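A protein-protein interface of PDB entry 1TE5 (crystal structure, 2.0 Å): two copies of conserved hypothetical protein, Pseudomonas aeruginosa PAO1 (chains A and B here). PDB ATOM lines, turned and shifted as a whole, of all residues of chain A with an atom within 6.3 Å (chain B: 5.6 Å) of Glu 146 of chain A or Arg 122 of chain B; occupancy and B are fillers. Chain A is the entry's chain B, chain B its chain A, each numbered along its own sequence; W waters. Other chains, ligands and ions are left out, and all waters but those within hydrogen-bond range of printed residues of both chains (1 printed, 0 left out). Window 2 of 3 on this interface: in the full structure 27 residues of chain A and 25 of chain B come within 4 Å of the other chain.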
ATOM      1  N   GLU A  97      23.595  23.838 -15.798  1.00  0.00           N
ATOM      2  CA  GLU A  97      22.582  23.663 -14.762  1.00  0.00           C
ATOM      3  C   GLU A  97      21.286  24.400 -15.087  1.00  0.00           C
ATOM      4  O   GLU A  97      21.300  25.557 -15.521  1.00  0.00           O
ATOM      5  CB  GLU A  97      23.093  24.081 -13.370  1.00  0.00           C
ATOM      6  CG  GLU A  97      23.064  25.582 -13.067  1.00  0.00           C
ATOM      7  CD  GLU A  97      21.816  26.068 -12.306  1.00  0.00           C
ATOM      8  OE1 GLU A  97      20.831  25.322 -12.132  1.00  0.00           O
ATOM      9  OE2 GLU A  97      21.826  27.229 -11.878  1.00  0.00           O
ATOM     10  N   LEU A  98      20.169  23.724 -14.862  1.00  0.00           N
ATOM     11  CA  LEU A  98      18.864  24.308 -15.100  1.00  0.00           C
ATOM     12  C   LEU A  98      17.982  23.830 -13.952  1.00  0.00           C
ATOM     13  O   LEU A  98      17.795  22.633 -13.760  1.00  0.00           O
ATOM     14  CB  LEU A  98      18.310  23.847 -16.461  1.00  0.00           C
ATOM     15  CG  LEU A  98      17.095  24.558 -17.091  1.00  0.00           C
ATOM     16  CD1 LEU A  98      16.868  24.031 -18.487  1.00  0.00           C
ATOM     17  CD2 LEU A  98      15.840  24.368 -16.275  1.00  0.00           C
ATOM     18  N   GLY A  99      17.471  24.769 -13.167  1.00  0.00           N
ATOM     19  CA  GLY A  99      16.611  24.410 -12.054  1.00  0.00           C
ATOM     20  C   GLY A  99      17.297  23.741 -10.878  1.00  0.00           C
ATOM     21  O   GLY A  99      16.637  23.045 -10.100  1.00  0.00           O
ATOM     22  N   GLY A 100      18.594  24.000 -10.706  1.00  0.00           N
ATOM     23  CA  GLY A 100      19.331  23.406  -9.603  1.00  0.00           C
ATOM     24  C   GLY A 100      19.731  21.961  -9.835  1.00  0.00           C
ATOM     25  O   GLY A 100      19.907  21.205  -8.882  1.00  0.00           O
ATOM     26  N   ARG A 101      19.869  21.581 -11.102  1.00  0.00           N
ATOM     27  CA  ARG A 101      20.277  20.235 -11.500  1.00  0.00           C
ATOM     28  C   ARG A 101      21.264  20.380 -12.653  1.00  0.00           C
ATOM     29  O   ARG A 101      21.183  21.335 -13.426  1.00  0.00           O
ATOM     30  CB  ARG A 101      19.078  19.417 -11.990  1.00  0.00           C
ATOM     31  CG  ARG A 101      17.899  19.308 -11.030  1.00  0.00           C
ATOM     32  CD  ARG A 101      18.236  18.542  -9.762  1.00  0.00           C
ATOM     33  NE  ARG A 101      18.802  17.219 -10.024  1.00  0.00           N
ATOM     34  CZ  ARG A 101      18.217  16.070  -9.701  1.00  0.00           C
ATOM     35  NH1 ARG A 101      18.821  14.925  -9.978  1.00  0.00           N
ATOM     36  NH2 ARG A 101      17.026  16.072  -9.113  1.00  0.00           N
ATOM     37  N   ARG A 141      13.594  26.484 -20.184  1.00  0.00           N
ATOM     38  CA  ARG A 141      13.599  27.550 -19.183  1.00  0.00           C
ATOM     39  C   ARG A 141      12.512  28.590 -19.442  1.00  0.00           C
ATOM     40  O   ARG A 141      12.002  29.207 -18.508  1.00  0.00           O
ATOM     41  CB  ARG A 141      14.967  28.242 -19.117  1.00  0.00           C
ATOM     42  CG  ARG A 141      15.029  29.416 -18.127  1.00  0.00           C
ATOM     43  CD  ARG A 141      16.479  29.878 -18.035  1.00  0.00           C
ATOM     44  NE  ARG A 141      17.020  29.768 -16.683  1.00  0.00           N
ATOM     45  CZ  ARG A 141      17.156  28.624 -16.014  1.00  0.00           C
ATOM     46  NH1 ARG A 141      17.657  28.625 -14.786  1.00  0.00           N
ATOM     47  NH2 ARG A 141      16.792  27.475 -16.569  1.00  0.00           N
ATOM     48  N   PHE A 144       9.211  26.658 -18.747  1.00  0.00           N
ATOM     49  CA  PHE A 144       9.162  26.238 -17.354  1.00  0.00           C
ATOM     50  C   PHE A 144      10.116  27.038 -16.474  1.00  0.00           C
ATOM     51  O   PHE A 144      11.210  26.570 -16.148  1.00  0.00           O
ATOM     52  CB  PHE A 144       9.487  24.745 -17.258  1.00  0.00           C
ATOM     53  CG  PHE A 144       8.672  23.892 -18.181  1.00  0.00           C
ATOM     54  CD1 PHE A 144       9.284  23.136 -19.170  1.00  0.00           C
ATOM     55  CD2 PHE A 144       7.285  23.883 -18.096  1.00  0.00           C
ATOM     56  CE1 PHE A 144       8.525  22.387 -20.062  1.00  0.00           C
ATOM     57  CE2 PHE A 144       6.522  23.139 -18.981  1.00  0.00           C
ATOM     58  CZ  PHE A 144       7.143  22.389 -19.968  1.00  0.00           C
ATOM     59  N   PRO A 145       9.708  28.257 -16.066  1.00  0.00           N
ATOM     60  CA  PRO A 145      10.528  29.126 -15.217  1.00  0.00           C
ATOM     61  C   PRO A 145      10.869  28.456 -13.889  1.00  0.00           C
ATOM     62  O   PRO A 145      11.917  28.713 -13.308  1.00  0.00           O
ATOM     63  CB  PRO A 145       9.626  30.344 -14.999  1.00  0.00           C
ATOM     64  CG  PRO A 145       8.764  30.363 -16.220  1.00  0.00           C
ATOM     65  CD  PRO A 145       8.427  28.912 -16.392  1.00  0.00           C
ATOM     66  N   GLU A 146       9.954  27.637 -13.387  1.00  0.00           N
ATOM     67  CA  GLU A 146      10.168  26.928 -12.132  1.00  0.00           C
ATOM     68  C   GLU A 146      10.218  25.426 -12.375  1.00  0.00           C
ATOM     69  O   GLU A 146       9.644  24.933 -13.347  1.00  0.00           O
ATOM     70  CB  GLU A 146       9.072  27.273 -11.121  1.00  0.00           C
ATOM     71  CG  GLU A 146       9.171  28.687 -10.560  1.00  0.00           C
ATOM     72  CD  GLU A 146      10.499  28.952  -9.877  1.00  0.00           C
ATOM     73  OE1 GLU A 146      10.886  28.166  -8.982  1.00  0.00           O
ATOM     74  OE2 GLU A 146      11.159  29.949 -10.242  1.00  0.00           O
ATOM     75  N   PRO A 147      10.953  24.689 -11.521  1.00  0.00           N
ATOM     76  CA  PRO A 147      11.100  23.235 -11.619  1.00  0.00           C
ATOM     77  C   PRO A 147       9.758  22.558 -11.794  1.00  0.00           C
ATOM     78  O   PRO A 147       8.815  22.833 -11.062  1.00  0.00           O
ATOM     79  CB  PRO A 147      11.751  22.883 -10.292  1.00  0.00           C
ATOM     80  CG  PRO A 147      12.674  24.040 -10.101  1.00  0.00           C
ATOM     81  CD  PRO A 147      11.772  25.213 -10.414  1.00  0.00           C
ATOM     82  N   VAL A 148       9.698  21.639 -12.747  1.00  0.00           N
ATOM     83  CA  VAL A 148       8.465  20.943 -13.066  1.00  0.00           C
ATOM     84  C   VAL A 148       8.740  19.454 -13.294  1.00  0.00           C
ATOM     85  O   VAL A 148       9.840  19.083 -13.716  1.00  0.00           O
ATOM     86  CB  VAL A 148       7.845  21.592 -14.341  1.00  0.00           C
ATOM     87  CG1 VAL A 148       8.183  20.810 -15.611  1.00  0.00           C
ATOM     88  CG2 VAL A 148       6.387  21.790 -14.172  1.00  0.00           C
ATOM     89  N   ARG B  96      29.700  27.286 -14.026  1.00  0.00           N
ATOM     90  CA  ARG B  96      28.435  27.723 -14.610  1.00  0.00           C
ATOM     91  C   ARG B  96      28.734  28.690 -15.744  1.00  0.00           C
ATOM     92  O   ARG B  96      29.595  29.561 -15.603  1.00  0.00           O
ATOM     93  CB  ARG B  96      27.545  28.379 -13.552  1.00  0.00           C
ATOM     94  CG  ARG B  96      26.113  27.879 -13.599  1.00  0.00           C
ATOM     95  CD  ARG B  96      25.482  27.740 -12.217  1.00  0.00           C
ATOM     96  NE  ARG B  96      26.208  26.706 -11.493  1.00  0.00           N
ATOM     97  CZ  ARG B  96      25.690  25.962 -10.522  1.00  0.00           C
ATOM     98  NH1 ARG B  96      26.444  25.059  -9.924  1.00  0.00           N
ATOM     99  NH2 ARG B  96      24.423  26.107 -10.150  1.00  0.00           N
ATOM    100  N   PRO B 118      16.280  33.567  -4.749  1.00  0.00           N
ATOM    101  CA  PRO B 118      16.407  32.622  -5.863  1.00  0.00           C
ATOM    102  C   PRO B 118      16.311  33.351  -7.199  1.00  0.00           C
ATOM    103  O   PRO B 118      15.462  34.231  -7.377  1.00  0.00           O
ATOM    104  CB  PRO B 118      15.222  31.691  -5.642  1.00  0.00           C
ATOM    105  CG  PRO B 118      15.113  31.660  -4.160  1.00  0.00           C
ATOM    106  CD  PRO B 118      15.236  33.121  -3.811  1.00  0.00           C
ATOM    107  N   GLY B 119      17.180  32.984  -8.133  1.00  0.00           N
ATOM    108  CA  GLY B 119      17.187  33.639  -9.425  1.00  0.00           C
ATOM    109  C   GLY B 119      17.448  32.692 -10.567  1.00  0.00           C
ATOM    110  O   GLY B 119      17.094  31.519 -10.487  1.00  0.00           O
ATOM    111  N   PHE B 120      18.018  33.228 -11.645  1.00  0.00           N
ATOM    112  CA  PHE B 120      18.348  32.476 -12.856  1.00  0.00           C
ATOM    113  C   PHE B 120      19.151  31.224 -12.520  1.00  0.00           C
ATOM    114  O   PHE B 120      18.837  30.121 -12.983  1.00  0.00           O
ATOM    115  CB  PHE B 120      19.198  33.328 -13.808  1.00  0.00           C
ATOM    116  CG  PHE B 120      18.659  34.713 -14.062  1.00  0.00           C
ATOM    117  CD1 PHE B 120      17.526  34.907 -14.862  1.00  0.00           C
ATOM    118  CD2 PHE B 120      19.324  35.836 -13.538  1.00  0.00           C
ATOM    119  CE1 PHE B 120      17.061  36.199 -15.138  1.00  0.00           C
ATOM    120  CE2 PHE B 120      18.875  37.130 -13.801  1.00  0.00           C
ATOM    121  CZ  PHE B 120      17.739  37.316 -14.608  1.00  0.00           C
ATOM    122  N   TYR B 121      20.261  31.432 -11.819  1.00  0.00           N
ATOM    123  CA  TYR B 121      21.138  30.351 -11.404  1.00  0.00           C
ATOM    124  C   TYR B 121      20.705  29.833 -10.042  1.00  0.00           C
ATOM    125  O   TYR B 121      20.394  30.606  -9.136  1.00  0.00           O
ATOM    126  CB  TYR B 121      22.588  30.835 -11.337  1.00  0.00           C
ATOM    127  CG  TYR B 121      23.145  31.324 -12.655  1.00  0.00           C
ATOM    128  CD1 TYR B 121      23.085  32.676 -13.003  1.00  0.00           C
ATOM    129  CD2 TYR B 121      23.752  30.443 -13.552  1.00  0.00           C
ATOM    130  CE1 TYR B 121      23.617  33.141 -14.207  1.00  0.00           C
ATOM    131  CE2 TYR B 121      24.290  30.900 -14.761  1.00  0.00           C
ATOM    132  CZ  TYR B 121      24.217  32.250 -15.077  1.00  0.00           C
ATOM    133  OH  TYR B 121      24.738  32.710 -16.264  1.00  0.00           O
ATOM    134  N   ARG B 122      20.672  28.515  -9.907  1.00  0.00           N
ATOM    135  CA  ARG B 122      20.289  27.891  -8.651  1.00  0.00           C
ATOM    136  C   ARG B 122      21.339  26.853  -8.262  1.00  0.00           C
ATOM    137  O   ARG B 122      21.920  26.190  -9.125  1.00  0.00           O
ATOM    138  CB  ARG B 122      18.917  27.221  -8.781  1.00  0.00           C
ATOM    139  CG  ARG B 122      17.790  28.156  -9.182  1.00  0.00           C
ATOM    140  CD  ARG B 122      16.457  27.441  -9.089  1.00  0.00           C
ATOM    141  NE  ARG B 122      15.352  28.242  -9.602  1.00  0.00           N
ATOM    142  CZ  ARG B 122      14.856  29.318  -9.005  1.00  0.00           C
ATOM    143  NH1 ARG B 122      13.849  29.975  -9.556  1.00  0.00           N
ATOM    144  NH2 ARG B 122      15.373  29.742  -7.862  1.00  0.00           N
ATOM    145  N   PRO B 123      21.665  26.767  -6.961  1.00  0.00           N
ATOM    146  CA  PRO B 123      22.660  25.776  -6.553  1.00  0.00           C
ATOM    147  C   PRO B 123      22.105  24.346  -6.660  1.00  0.00           C
ATOM    148  O   PRO B 123      20.894  24.115  -6.510  1.00  0.00           O
ATOM    149  CB  PRO B 123      22.957  26.177  -5.102  1.00  0.00           C
ATOM    150  CG  PRO B 123      21.674  26.748  -4.632  1.00  0.00           C
ATOM    151  CD  PRO B 123      21.252  27.599  -5.816  1.00  0.00           C
ATOM    152  N   VAL B 124      22.986  23.415  -7.009  1.00  0.00           N
ATOM    153  CA  VAL B 124      22.629  22.001  -7.106  1.00  0.00           C
ATOM    154  C   VAL B 124      22.834  21.364  -5.716  1.00  0.00           C
ATOM    155  O   VAL B 124      22.080  20.475  -5.298  1.00  0.00           O
ATOM    156  CB  VAL B 124      23.505  21.286  -8.159  1.00  0.00           C
ATOM    157  CG1 VAL B 124      23.126  19.812  -8.250  1.00  0.00           C
ATOM    158  CG2 VAL B 124      23.337  21.968  -9.517  1.00  0.00           C
ATOM    159  N   GLU B 130      28.114  27.767  -2.945  1.00  0.00           N
ATOM    160  CA  GLU B 130      27.426  27.677  -4.228  1.00  0.00           C
ATOM    161  C   GLU B 130      26.254  28.650  -4.314  1.00  0.00           C
ATOM    162  O   GLU B 130      25.921  29.139  -5.395  1.00  0.00           O
ATOM    163  CB  GLU B 130      26.951  26.250  -4.478  1.00  0.00           C
ATOM    164  CG  GLU B 130      26.340  26.039  -5.844  1.00  0.00           C
ATOM    165  CD  GLU B 130      25.990  24.598  -6.113  1.00  0.00           C
ATOM    166  OE1 GLU B 130      26.069  23.769  -5.174  1.00  0.00           O
ATOM    167  OE2 GLU B 130      25.643  24.298  -7.277  1.00  0.00           O
ATOM    168  N   CYS B 134      26.016  31.426  -7.356  1.00  0.00           N
ATOM    169  CA  CYS B 134      24.848  31.651  -8.181  1.00  0.00           C
ATOM    170  C   CYS B 134      24.325  33.066  -8.016  1.00  0.00           C
ATOM    171  O   CYS B 134      24.033  33.723  -9.006  1.00  0.00           O
ATOM    172  CB  CYS B 134      23.760  30.651  -7.830  1.00  0.00           C
ATOM    173  SG  CYS B 134      24.219  28.968  -8.231  1.00  0.00           S
HETATM  174  O   HOH W   1      19.129  20.185  -6.270  1.00  0.00           O
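NH1 of Arg 122 of chain B is in salt-bridge range of OE2 of Glu 146 of chain A, 2.8 Å away.
The guanidinium group of Arg 141 of chain A is in hydrogen-bond range of the backbone carbonyl oxygen of Phe 120 of chain B (2.6 Å).
The backbone NH (N) of Arg 122 of chain B sits at hydrogen-bond distance from the side-chain carboxylate (OE2) of Glu 97 of chain A, 2.6 Å away.
The side-chain carboxylate of Glu 97 of chain A lies within salt-bridge range of the guanidinium group of Arg 96 of chain B (3.3 Å).
The guanidinium group (NH2) of Arg 96 of chain B is in hydrogen-bond range of the side-chain sulfur (SG) of Cys 134 of chain B, at 3.5 Å.
The backbone NH of Val 124 of chain B lies within hydrogen-bond range of the side-chain carboxylate of Glu 130 of chain B, 2.8 Å away.
The side-chain carboxylate of Glu 97 of chain A lies within hydrogen-bond range of the backbone NH of Gly 100 of chain A (3.0 Å).
NH2 of Arg 96 of chain B lies within hydrogen-bond range of O of Arg 122 of chain B (2.7 Å).
The backbone carbonyl oxygen (O) of Arg 122 of chain B lies close to the side-chain sulfur (SG) of Cys 134 of chain B (3.7 Å).
The side-chain carboxylate (OE2) of Glu 130 of chain B lies within salt-bridge range of the guanidinium group (NH1) of Arg 96 of chain B (2.9 Å).
Among the printed residues, pairs that only touch across the chains: Glu 97 of chain A with Tyr 121 of chain B, Gly 100 of chain A with Val 124 of chain B, Gly 100 of chain A with Pro 123 of chain B, Gly 100 of chain A with Arg 122 of chain B and Arg 101 of chain A with Val 124 of chain B.
Of the printed residues of chain B, Glu 97 of chain A touches Arg 96, Tyr 121 and Arg 122.
Gly 99 of chain A touches none of the printed residues of chain B.
Of the printed residues of chain B, Arg 101 of chain A touches Val 124.
Printed residues of chain B within 4 Å of Glu 146 of chain A: Arg 122.
Printed residues of chain A within 4 Å of Arg 96 of chain B: Glu 97.
Printed residues of chain A within 4 Å of Tyr 121 of chain B: Glu 97.
Of chain A, only Glu 97, Gly 100 and Glu 146 come within 4 Å of Arg 122 of chain B.
Of the 11 printed residues of chain A, 5 touch a printed residue of chain B.
Hydrophobic or aromatic side chains of chain B that line the printed part of chain A: Tyr 121 and Val 124.
Among the printed residues, 9 pairs touch across the chains.
Among the printed residues, Asp or Glu carboxylates within 4 Å of a Lys or Arg side-chain nitrogen of the other chain: Glu 97 of chain A with Arg 96 of chain B (3.3 Å) and Glu 146 of chain A with Arg 122 of chain B (2.8 Å).
No position is printed for both chains.
Of the 9 pairs that touch across the chains among the printed residues, none has its exchanged pair printed and touching as well.
Water W1 bridges the backbone carbonyl oxygen (O) of Gly 100 of chain A and the backbone carbonyl oxygen (O) of Val 124 of chain B.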
